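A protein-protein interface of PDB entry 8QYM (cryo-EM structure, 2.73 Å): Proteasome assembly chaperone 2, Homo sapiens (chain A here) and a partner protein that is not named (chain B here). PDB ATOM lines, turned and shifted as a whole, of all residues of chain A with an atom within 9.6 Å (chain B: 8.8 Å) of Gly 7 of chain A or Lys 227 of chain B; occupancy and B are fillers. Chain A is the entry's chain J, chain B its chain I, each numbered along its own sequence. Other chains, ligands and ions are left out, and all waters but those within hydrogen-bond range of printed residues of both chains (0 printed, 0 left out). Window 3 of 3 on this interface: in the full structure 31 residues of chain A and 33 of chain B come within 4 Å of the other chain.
NZ of Lys 227 of chain B touches O of Pro 5 of chain A, 3.7 Å away. Cys 6 of chain A touches Lys 227 of chain B. Lys 227 of chain B touches Gly 7 of chain A.
O of Val 4 of chain A lies within hydrogen-bond range of N of Tyr 47 of chain A (2.8 Å). The side-chain sulfur (SG) of Cys 6 of chain A sits at hydrogen-bond distance from the backbone NH (N) of Gly 46 of chain A, 3.6 Å away. O of Ile 45 of chain A sits at hydrogen-bond distance from N of Cys 6 of chain A (3.1 Å). The side-chain amino group (NZ) of Lys 44 of chain A sits at hydrogen-bond distance from the side-chain hydroxyl (OH) of Tyr 47 of chain A, 3.5 Å away.
The side-chain hydroxyl (OH) of Tyr 47 of chain A lies within hydrogen-bond range of the side-chain amide nitrogen (NE2) of Gln 224 of chain B.
Gly 7 of chain A touches one residue of chain B. Of the printed residues of chain A, Lys 227 of chain B touches Pro 5, Cys 6 and Gly 7. No residue of chain A comes within 4 Å of Lys 160 of chain B. No residue of chain A comes within 4 Å of Ile 228 of chain B. Printed residues of chain B within 4 Å of Cys 6 of chain A: Lys 227 (3.4 Å). Of the printed residues of chain B, Tyr 47 of chain A touches Gln 224 (3.2 Å). Of the printed residues of chain B, Pro 5 of chain A touches Lys 227. Of the printed residues of chain A, Gln 224 of chain B touches Tyr 47 (3.2 Å). Ala 230 of chain B touches none of the printed residues of chain A. The nearest residue of chain B that does not touch Gly 7 of chain A is Gln 195 of chain B (7.4 Å). The nearest residue of chain A that does not touch Lys 227 of chain B is Val 4 of chain A (5.3 Å).
Of the 20 printed residues of chain B, 2 touch a printed residue of chain A. Along chain A the printed residues that touch a printed residue of chain B span positions 5 to 47. Among the printed residues, no Asp or Glu carboxylate lies within 4 Å of a Lys or Arg side-chain nitrogen of the other chain.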
ATOM      1  N   PHE A   3       2.610  19.324 -19.411  1.00  0.00           N
ATOM      2  CA  PHE A   3       1.279  19.699 -19.911  1.00  0.00           C
ATOM      3  C   PHE A   3       0.976  18.955 -21.204  1.00  0.00           C
ATOM      4  O   PHE A   3       1.693  19.176 -22.182  1.00  0.00           O
ATOM      5  CB  PHE A   3       1.126  21.205 -20.085  1.00  0.00           C
ATOM      6  CG  PHE A   3      -0.229  21.688 -20.526  1.00  0.00           C
ATOM      7  CD1 PHE A   3      -1.246  21.861 -19.609  1.00  0.00           C
ATOM      8  CD2 PHE A   3      -0.478  21.995 -21.851  1.00  0.00           C
ATOM      9  CE1 PHE A   3      -2.491  22.310 -20.011  1.00  0.00           C
ATOM     10  CE2 PHE A   3      -1.724  22.442 -22.253  1.00  0.00           C
ATOM     11  CZ  PHE A   3      -2.726  22.605 -21.331  1.00  0.00           C
ATOM     12  N   VAL A   4      -0.044  18.106 -21.183  1.00  0.00           N
ATOM     13  CA  VAL A   4      -0.573  17.403 -22.345  1.00  0.00           C
ATOM     14  C   VAL A   4      -1.880  18.085 -22.747  1.00  0.00           C
ATOM     15  O   VAL A   4      -2.864  18.025 -21.995  1.00  0.00           O
ATOM     16  CB  VAL A   4      -0.789  15.912 -22.058  1.00  0.00           C
ATOM     17  CG1 VAL A   4      -1.041  15.158 -23.350  1.00  0.00           C
ATOM     18  CG2 VAL A   4       0.409  15.335 -21.325  1.00  0.00           C
ATOM     19  N   PRO A   5      -1.941  18.740 -23.903  1.00  0.00           N
ATOM     20  CA  PRO A   5      -3.179  19.413 -24.306  1.00  0.00           C
ATOM     21  C   PRO A   5      -4.298  18.427 -24.600  1.00  0.00           C
ATOM     22  O   PRO A   5      -4.067  17.304 -25.055  1.00  0.00           O
ATOM     23  CB  PRO A   5      -2.772  20.178 -25.570  1.00  0.00           C
ATOM     24  CG  PRO A   5      -1.599  19.426 -26.098  1.00  0.00           C
ATOM     25  CD  PRO A   5      -0.867  18.916 -24.895  1.00  0.00           C
ATOM     26  N   CYS A   6      -5.529  18.865 -24.329  1.00  0.00           N
ATOM     27  CA  CYS A   6      -6.694  18.049 -24.657  1.00  0.00           C
ATOM     28  C   CYS A   6      -6.853  17.896 -26.164  1.00  0.00           C
ATOM     29  O   CYS A   6      -7.188  16.811 -26.651  1.00  0.00           O
ATOM     30  CB  CYS A   6      -7.954  18.659 -24.044  1.00  0.00           C
ATOM     31  SG  CYS A   6      -8.138  18.378 -22.270  1.00  0.00           S
ATOM     32  N   GLY A   7      -6.622  18.970 -26.915  1.00  0.00           N
ATOM     33  CA  GLY A   7      -6.743  18.928 -28.359  1.00  0.00           C
ATOM     34  C   GLY A   7      -5.457  18.530 -29.052  1.00  0.00           C
ATOM     35  O   GLY A   7      -4.863  17.497 -28.730  1.00  0.00           O
ATOM     36  N   GLU A   8      -5.016  19.343 -30.011  1.00  0.00           N
ATOM     37  CA  GLU A   8      -3.806  19.061 -30.770  1.00  0.00           C
ATOM     38  C   GLU A   8      -2.681  20.053 -30.525  1.00  0.00           C
ATOM     39  O   GLU A   8      -1.514  19.690 -30.678  1.00  0.00           O
ATOM     40  CB  GLU A   8      -4.115  19.029 -32.273  1.00  0.00           C
ATOM     41  N   SER A   9      -2.997  21.291 -30.151  1.00  0.00           N
ATOM     42  CA  SER A   9      -1.993  22.322 -29.928  1.00  0.00           C
ATOM     43  C   SER A   9      -2.201  22.955 -28.561  1.00  0.00           C
ATOM     44  O   SER A   9      -3.337  23.210 -28.151  1.00  0.00           O
ATOM     45  CB  SER A   9      -2.053  23.398 -31.018  1.00  0.00           C
ATOM     46  OG  SER A   9      -3.387  23.815 -31.251  1.00  0.00           O
ATOM     47  N   ALA A  10      -1.099  23.203 -27.862  1.00  0.00           N
ATOM     48  CA  ALA A  10      -1.178  23.827 -26.551  1.00  0.00           C
ATOM     49  C   ALA A  10      -1.628  25.280 -26.683  1.00  0.00           C
ATOM     50  O   ALA A  10      -1.182  25.989 -27.591  1.00  0.00           O
ATOM     51  CB  ALA A  10       0.173  23.760 -25.842  1.00  0.00           C
ATOM     52  N   PRO A  11      -2.507  25.750 -25.802  1.00  0.00           N
ATOM     53  CA  PRO A  11      -2.936  27.151 -25.864  1.00  0.00           C
ATOM     54  C   PRO A  11      -1.811  28.093 -25.467  1.00  0.00           C
ATOM     55  O   PRO A  11      -0.854  27.720 -24.784  1.00  0.00           O
ATOM     56  CB  PRO A  11      -4.093  27.213 -24.862  1.00  0.00           C
ATOM     57  CG  PRO A  11      -3.818  26.108 -23.907  1.00  0.00           C
ATOM     58  CD  PRO A  11      -3.143  25.020 -24.693  1.00  0.00           C
ATOM     59  N   LYS A  44     -11.814  23.272 -19.398  1.00  0.00           N
ATOM     60  CA  LYS A  44     -10.610  22.454 -19.367  1.00  0.00           C
ATOM     61  C   LYS A  44      -9.807  22.621 -20.651  1.00  0.00           C
ATOM     62  O   LYS A  44     -10.367  22.716 -21.746  1.00  0.00           O
ATOM     63  CB  LYS A  44     -10.974  20.984 -19.166  1.00  0.00           C
ATOM     64  CG  LYS A  44      -9.882  20.158 -18.512  1.00  0.00           C
ATOM     65  CD  LYS A  44     -10.006  18.692 -18.880  1.00  0.00           C
ATOM     66  CE  LYS A  44     -11.366  18.143 -18.494  1.00  0.00           C
ATOM     67  NZ  LYS A  44     -11.360  16.657 -18.413  1.00  0.00           N
ATOM     68  N   ILE A  45      -8.482  22.656 -20.512  1.00  0.00           N
ATOM     69  CA  ILE A  45      -7.600  22.815 -21.665  1.00  0.00           C
ATOM     70  C   ILE A  45      -6.521  21.749 -21.756  1.00  0.00           C
ATOM     71  O   ILE A  45      -5.926  21.576 -22.835  1.00  0.00           O
ATOM     72  CB  ILE A  45      -6.956  24.220 -21.671  1.00  0.00           C
ATOM     73  CG1 ILE A  45      -6.186  24.462 -20.373  1.00  0.00           C
ATOM     74  CG2 ILE A  45      -8.008  25.294 -21.889  1.00  0.00           C
ATOM     75  CD1 ILE A  45      -5.140  25.544 -20.480  1.00  0.00           C
ATOM     76  N   GLY A  46      -6.211  21.011 -20.697  1.00  0.00           N
ATOM     77  CA  GLY A  46      -5.144  20.035 -20.787  1.00  0.00           C
ATOM     78  C   GLY A  46      -4.996  19.249 -19.504  1.00  0.00           C
ATOM     79  O   GLY A  46      -5.823  19.336 -18.595  1.00  0.00           O
ATOM     80  N   TYR A  47      -3.914  18.474 -19.451  1.00  0.00           N
ATOM     81  CA  TYR A  47      -3.609  17.592 -18.335  1.00  0.00           C
ATOM     82  C   TYR A  47      -2.187  17.845 -17.859  1.00  0.00           C
ATOM     83  O   TYR A  47      -1.322  18.264 -18.633  1.00  0.00           O
ATOM     84  CB  TYR A  47      -3.753  16.115 -18.730  1.00  0.00           C
ATOM     85  CG  TYR A  47      -5.165  15.689 -19.053  1.00  0.00           C
ATOM     86  CD1 TYR A  47      -6.166  15.750 -18.095  1.00  0.00           C
ATOM     87  CD2 TYR A  47      -5.499  15.239 -20.322  1.00  0.00           C
ATOM     88  CE1 TYR A  47      -7.456  15.363 -18.387  1.00  0.00           C
ATOM     89  CE2 TYR A  47      -6.788  14.854 -20.624  1.00  0.00           C
ATOM     90  CZ  TYR A  47      -7.761  14.917 -19.654  1.00  0.00           C
ATOM     91  OH  TYR A  47      -9.048  14.534 -19.950  1.00  0.00           O
ATOM     92  N   PRO B 158       2.760   4.982 -27.385  1.00  0.00           N
ATOM     93  CA  PRO B 158       1.357   4.557 -27.432  1.00  0.00           C
ATOM     94  C   PRO B 158       0.872   4.342 -28.856  1.00  0.00           C
ATOM     95  O   PRO B 158       1.307   5.006 -29.799  1.00  0.00           O
ATOM     96  CB  PRO B 158       0.605   5.716 -26.761  1.00  0.00           C
ATOM     97  CG  PRO B 158       1.657   6.612 -26.173  1.00  0.00           C
ATOM     98  CD  PRO B 158       2.906   6.377 -26.947  1.00  0.00           C
ATOM     99  N   ARG B 159      -0.046   3.390 -29.000  1.00  0.00           N
ATOM    100  CA  ARG B 159      -0.739   3.130 -30.255  1.00  0.00           C
ATOM    101  C   ARG B 159      -2.221   3.396 -30.040  1.00  0.00           C
ATOM    102  O   ARG B 159      -2.838   2.799 -29.152  1.00  0.00           O
ATOM    103  CB  ARG B 159      -0.508   1.693 -30.727  1.00  0.00           C
ATOM    104  CG  ARG B 159       0.928   1.395 -31.121  1.00  0.00           C
ATOM    105  CD  ARG B 159       1.215  -0.097 -31.076  1.00  0.00           C
ATOM    106  NE  ARG B 159       2.513  -0.422 -31.654  1.00  0.00           N
ATOM    107  CZ  ARG B 159       3.112  -1.599 -31.538  1.00  0.00           C
ATOM    108  NH1 ARG B 159       2.558  -2.591 -30.862  1.00  0.00           N
ATOM    109  NH2 ARG B 159       4.295  -1.785 -32.115  1.00  0.00           N
ATOM    110  N   LYS B 160      -2.789   4.290 -30.848  1.00  0.00           N
ATOM    111  CA  LYS B 160      -4.178   4.689 -30.663  1.00  0.00           C
ATOM    112  C   LYS B 160      -5.165   3.746 -31.336  1.00  0.00           C
ATOM    113  O   LYS B 160      -6.376   3.903 -31.140  1.00  0.00           O
ATOM    114  CB  LYS B 160      -4.384   6.115 -31.182  1.00  0.00           C
ATOM    115  CG  LYS B 160      -3.465   7.140 -30.534  1.00  0.00           C
ATOM    116  CD  LYS B 160      -4.097   8.523 -30.497  1.00  0.00           C
ATOM    117  CE  LYS B 160      -4.400   9.033 -31.896  1.00  0.00           C
ATOM    118  NZ  LYS B 160      -5.058  10.368 -31.867  1.00  0.00           N
ATOM    119  N   ASN B 161      -4.691   2.781 -32.116  1.00  0.00           N
ATOM    120  CA  ASN B 161      -5.560   1.787 -32.745  1.00  0.00           C
ATOM    121  C   ASN B 161      -5.609   0.510 -31.905  1.00  0.00           C
ATOM    122  O   ASN B 161      -5.223  -0.578 -32.330  1.00  0.00           O
ATOM    123  CB  ASN B 161      -5.096   1.511 -34.174  1.00  0.00           C
ATOM    124  CG  ASN B 161      -3.681   0.966 -34.238  1.00  0.00           C
ATOM    125  OD1 ASN B 161      -2.951   0.978 -33.246  1.00  0.00           O
ATOM    126  ND2 ASN B 161      -3.286   0.482 -35.410  1.00  0.00           N
ATOM    127  N   MET B 162      -6.116   0.664 -30.684  1.00  0.00           N
ATOM    128  CA  MET B 162      -6.144  -0.429 -29.724  1.00  0.00           C
ATOM    129  C   MET B 162      -7.260  -0.178 -28.721  1.00  0.00           C
ATOM    130  O   MET B 162      -7.446   0.953 -28.266  1.00  0.00           O
ATOM    131  CB  MET B 162      -4.793  -0.563 -29.010  1.00  0.00           C
ATOM    132  CG  MET B 162      -4.706  -1.712 -28.025  1.00  0.00           C
ATOM    133  SD  MET B 162      -3.082  -1.819 -27.250  1.00  0.00           S
ATOM    134  CE  MET B 162      -3.124  -0.393 -26.170  1.00  0.00           C
ATOM    135  N   THR B 194     -13.642   6.461 -21.568  1.00  0.00           N
ATOM    136  CA  THR B 194     -12.802   7.570 -21.994  1.00  0.00           C
ATOM    137  C   THR B 194     -13.523   8.352 -23.092  1.00  0.00           C
ATOM    138  O   THR B 194     -14.681   8.082 -23.423  1.00  0.00           O
ATOM    139  CB  THR B 194     -11.437   7.069 -22.464  1.00  0.00           C
ATOM    140  OG1 THR B 194     -11.585   6.359 -23.698  1.00  0.00           O
ATOM    141  CG2 THR B 194     -10.821   6.150 -21.425  1.00  0.00           C
ATOM    142  N   GLN B 195     -12.837   9.336 -23.675  1.00  0.00           N
ATOM    143  CA  GLN B 195     -13.469  10.204 -24.661  1.00  0.00           C
ATOM    144  C   GLN B 195     -13.630   9.530 -26.018  1.00  0.00           C
ATOM    145  O   GLN B 195     -14.598   9.814 -26.732  1.00  0.00           O
ATOM    146  CB  GLN B 195     -12.660  11.492 -24.815  1.00  0.00           C
ATOM    147  CG  GLN B 195     -13.407  12.620 -25.499  1.00  0.00           C
ATOM    148  CD  GLN B 195     -12.487  13.741 -25.936  1.00  0.00           C
ATOM    149  OE1 GLN B 195     -12.667  14.895 -25.548  1.00  0.00           O
ATOM    150  NE2 GLN B 195     -11.491  13.407 -26.748  1.00  0.00           N
ATOM    151  N   ASN B 196     -12.709   8.644 -26.390  1.00  0.00           N
ATOM    152  CA  ASN B 196     -12.700   8.046 -27.718  1.00  0.00           C
ATOM    153  C   ASN B 196     -13.534   6.776 -27.819  1.00  0.00           C
ATOM    154  O   ASN B 196     -13.644   6.214 -28.912  1.00  0.00           O
ATOM    155  CB  ASN B 196     -11.261   7.749 -28.148  1.00  0.00           C
ATOM    156  CG  ASN B 196     -10.533   8.983 -28.634  1.00  0.00           C
ATOM    157  OD1 ASN B 196     -11.086  10.082 -28.638  1.00  0.00           O
ATOM    158  ND2 ASN B 196      -9.285   8.809 -29.052  1.00  0.00           N
ATOM    159  N   PHE B 197     -14.119   6.307 -26.720  1.00  0.00           N
ATOM    160  CA  PHE B 197     -14.958   5.112 -26.749  1.00  0.00           C
ATOM    161  C   PHE B 197     -16.312   5.496 -27.331  1.00  0.00           C
ATOM    162  O   PHE B 197     -17.164   6.059 -26.640  1.00  0.00           O
ATOM    163  CB  PHE B 197     -15.098   4.516 -25.354  1.00  0.00           C
ATOM    164  CG  PHE B 197     -15.513   3.073 -25.352  1.00  0.00           C
ATOM    165  CD1 PHE B 197     -14.583   2.072 -25.568  1.00  0.00           C
ATOM    166  CD2 PHE B 197     -16.832   2.717 -25.135  1.00  0.00           C
ATOM    167  CE1 PHE B 197     -14.959   0.745 -25.566  1.00  0.00           C
ATOM    168  CE2 PHE B 197     -17.213   1.392 -25.132  1.00  0.00           C
ATOM    169  CZ  PHE B 197     -16.276   0.405 -25.349  1.00  0.00           C
ATOM    170  N   LEU B 220      -6.999   3.434 -16.737  1.00  0.00           N
ATOM    171  CA  LEU B 220      -7.967   4.318 -17.376  1.00  0.00           C
ATOM    172  C   LEU B 220      -7.400   5.720 -17.558  1.00  0.00           C
ATOM    173  O   LEU B 220      -7.642   6.364 -18.584  1.00  0.00           O
ATOM    174  CB  LEU B 220      -9.262   4.361 -16.565  1.00  0.00           C
ATOM    175  CG  LEU B 220     -10.526   4.719 -17.351  1.00  0.00           C
ATOM    176  CD1 LEU B 220     -10.747   3.742 -18.490  1.00  0.00           C
ATOM    177  CD2 LEU B 220     -11.734   4.753 -16.438  1.00  0.00           C
ATOM    178  N   SER B 221      -6.645   6.212 -16.572  1.00  0.00           N
ATOM    179  CA  SER B 221      -6.021   7.524 -16.695  1.00  0.00           C
ATOM    180  C   SER B 221      -5.009   7.548 -17.830  1.00  0.00           C
ATOM    181  O   SER B 221      -4.946   8.518 -18.595  1.00  0.00           O
ATOM    182  CB  SER B 221      -5.352   7.910 -15.377  1.00  0.00           C
ATOM    183  OG  SER B 221      -6.284   7.904 -14.312  1.00  0.00           O
ATOM    184  N   TYR B 222      -4.200   6.493 -17.950  1.00  0.00           N
ATOM    185  CA  TYR B 222      -3.250   6.406 -19.055  1.00  0.00           C
ATOM    186  C   TYR B 222      -3.973   6.457 -20.395  1.00  0.00           C
ATOM    187  O   TYR B 222      -3.596   7.220 -21.295  1.00  0.00           O
ATOM    188  CB  TYR B 222      -2.427   5.123 -18.929  1.00  0.00           C
ATOM    189  CG  TYR B 222      -1.353   4.949 -19.979  1.00  0.00           C
ATOM    190  CD1 TYR B 222      -1.634   4.350 -21.200  1.00  0.00           C
ATOM    191  CD2 TYR B 222      -0.052   5.369 -19.742  1.00  0.00           C
ATOM    192  CE1 TYR B 222      -0.654   4.188 -22.158  1.00  0.00           C
ATOM    193  CE2 TYR B 222       0.934   5.208 -20.694  1.00  0.00           C
ATOM    194  CZ  TYR B 222       0.627   4.618 -21.899  1.00  0.00           C
ATOM    195  OH  TYR B 222       1.608   4.458 -22.850  1.00  0.00           O
ATOM    196  N   CYS B 223      -5.032   5.655 -20.538  1.00  0.00           N
ATOM    197  CA  CYS B 223      -5.764   5.621 -21.799  1.00  0.00           C
ATOM    198  C   CYS B 223      -6.402   6.970 -22.110  1.00  0.00           C
ATOM    199  O   CYS B 223      -6.387   7.420 -23.262  1.00  0.00           O
ATOM    200  CB  CYS B 223      -6.823   4.520 -21.761  1.00  0.00           C
ATOM    201  SG  CYS B 223      -6.151   2.847 -21.694  1.00  0.00           S
ATOM    202  N   GLN B 224      -6.976   7.627 -21.099  1.00  0.00           N
ATOM    203  CA  GLN B 224      -7.603   8.926 -21.319  1.00  0.00           C
ATOM    204  C   GLN B 224      -6.579   9.981 -21.717  1.00  0.00           C
ATOM    205  O   GLN B 224      -6.829  10.786 -22.621  1.00  0.00           O
ATOM    206  CB  GLN B 224      -8.360   9.362 -20.065  1.00  0.00           C
ATOM    207  CG  GLN B 224      -8.814  10.814 -20.078  1.00  0.00           C
ATOM    208  CD  GLN B 224     -10.052  11.034 -20.925  1.00  0.00           C
ATOM    209  OE1 GLN B 224     -11.036  10.308 -20.805  1.00  0.00           O
ATOM    210  NE2 GLN B 224     -10.008  12.042 -21.784  1.00  0.00           N
ATOM    211  N   VAL B 225      -5.420   9.994 -21.054  1.00  0.00           N
ATOM    212  CA  VAL B 225      -4.408  11.000 -21.352  1.00  0.00           C
ATOM    213  C   VAL B 225      -3.843  10.799 -22.753  1.00  0.00           C
ATOM    214  O   VAL B 225      -3.661  11.765 -23.504  1.00  0.00           O
ATOM    215  CB  VAL B 225      -3.301  10.976 -20.283  1.00  0.00           C
ATOM    216  CG1 VAL B 225      -2.093  11.766 -20.750  1.00  0.00           C
ATOM    217  CG2 VAL B 225      -3.823  11.533 -18.972  1.00  0.00           C
ATOM    218  N   TRP B 226      -3.571   9.552 -23.135  1.00  0.00           N
ATOM    219  CA  TRP B 226      -2.911   9.277 -24.405  1.00  0.00           C
ATOM    220  C   TRP B 226      -3.882   8.936 -25.531  1.00  0.00           C
ATOM    221  O   TRP B 226      -3.452   8.425 -26.569  1.00  0.00           O
ATOM    222  CB  TRP B 226      -1.881   8.161 -24.229  1.00  0.00           C
ATOM    223  CG  TRP B 226      -0.727   8.588 -23.378  1.00  0.00           C
ATOM    224  CD1 TRP B 226      -0.334   8.039 -22.195  1.00  0.00           C
ATOM    225  CD2 TRP B 226       0.173   9.674 -23.635  1.00  0.00           C
ATOM    226  NE1 TRP B 226       0.760   8.708 -21.703  1.00  0.00           N
ATOM    227  CE2 TRP B 226       1.090   9.716 -22.568  1.00  0.00           C
ATOM    228  CE3 TRP B 226       0.294  10.610 -24.666  1.00  0.00           C
ATOM    229  CZ2 TRP B 226       2.114  10.657 -22.503  1.00  0.00           C
ATOM    230  CZ3 TRP B 226       1.310  11.544 -24.599  1.00  0.00           C
ATOM    231  CH2 TRP B 226       2.206  11.560 -23.526  1.00  0.00           C
ATOM    232  N   LYS B 227      -5.176   9.204 -25.346  1.00  0.00           N
ATOM    233  CA  LYS B 227      -6.182   9.101 -26.406  1.00  0.00           C
ATOM    234  C   LYS B 227      -6.286   7.675 -26.951  1.00  0.00           C
ATOM    235  O   LYS B 227      -6.158   7.424 -28.150  1.00  0.00           O
ATOM    236  CB  LYS B 227      -5.889  10.098 -27.534  1.00  0.00           C
ATOM    237  CG  LYS B 227      -5.978  11.555 -27.122  1.00  0.00           C
ATOM    238  CD  LYS B 227      -5.872  12.469 -28.329  1.00  0.00           C
ATOM    239  CE  LYS B 227      -5.869  13.930 -27.915  1.00  0.00           C
ATOM    240  NZ  LYS B 227      -4.701  14.261 -27.055  1.00  0.00           N
ATOM    241  N   ILE B 228      -6.535   6.738 -26.043  1.00  0.00           N
ATOM    242  CA  ILE B 228      -6.738   5.335 -26.378  1.00  0.00           C
ATOM    243  C   ILE B 228      -8.137   4.949 -25.920  1.00  0.00           C
ATOM    244  O   ILE B 228      -8.494   5.217 -24.771  1.00  0.00           O
ATOM    245  CB  ILE B 228      -5.691   4.414 -25.726  1.00  0.00           C
ATOM    246  CG1 ILE B 228      -4.278   4.851 -26.118  1.00  0.00           C
ATOM    247  CG2 ILE B 228      -5.930   2.970 -26.123  1.00  0.00           C
ATOM    248  CD1 ILE B 228      -3.188   4.100 -25.391  1.00  0.00           C
ATOM    249  N   PRO B 229      -8.963   4.348 -26.775  1.00  0.00           N
ATOM    250  CA  PRO B 229     -10.288   3.905 -26.327  1.00  0.00           C
ATOM    251  C   PRO B 229     -10.177   2.867 -25.220  1.00  0.00           C
ATOM    252  O   PRO B 229      -9.330   1.972 -25.266  1.00  0.00           O
ATOM    253  CB  PRO B 229     -10.912   3.311 -27.595  1.00  0.00           C
ATOM    254  CG  PRO B 229     -10.155   3.932 -28.721  1.00  0.00           C
ATOM    255  CD  PRO B 229      -8.762   4.126 -28.217  1.00  0.00           C
ATOM    256  N   ALA B 230     -11.048   2.989 -24.223  1.00  0.00           N
ATOM    257  CA  ALA B 230     -11.027   2.081 -23.085  1.00  0.00           C
ATOM    258  C   ALA B 230     -12.368   2.145 -22.372  1.00  0.00           C
ATOM    259  O   ALA B 230     -13.153   3.077 -22.566  1.00  0.00           O
ATOM    260  CB  ALA B 230      -9.886   2.414 -22.119  1.00  0.00           C
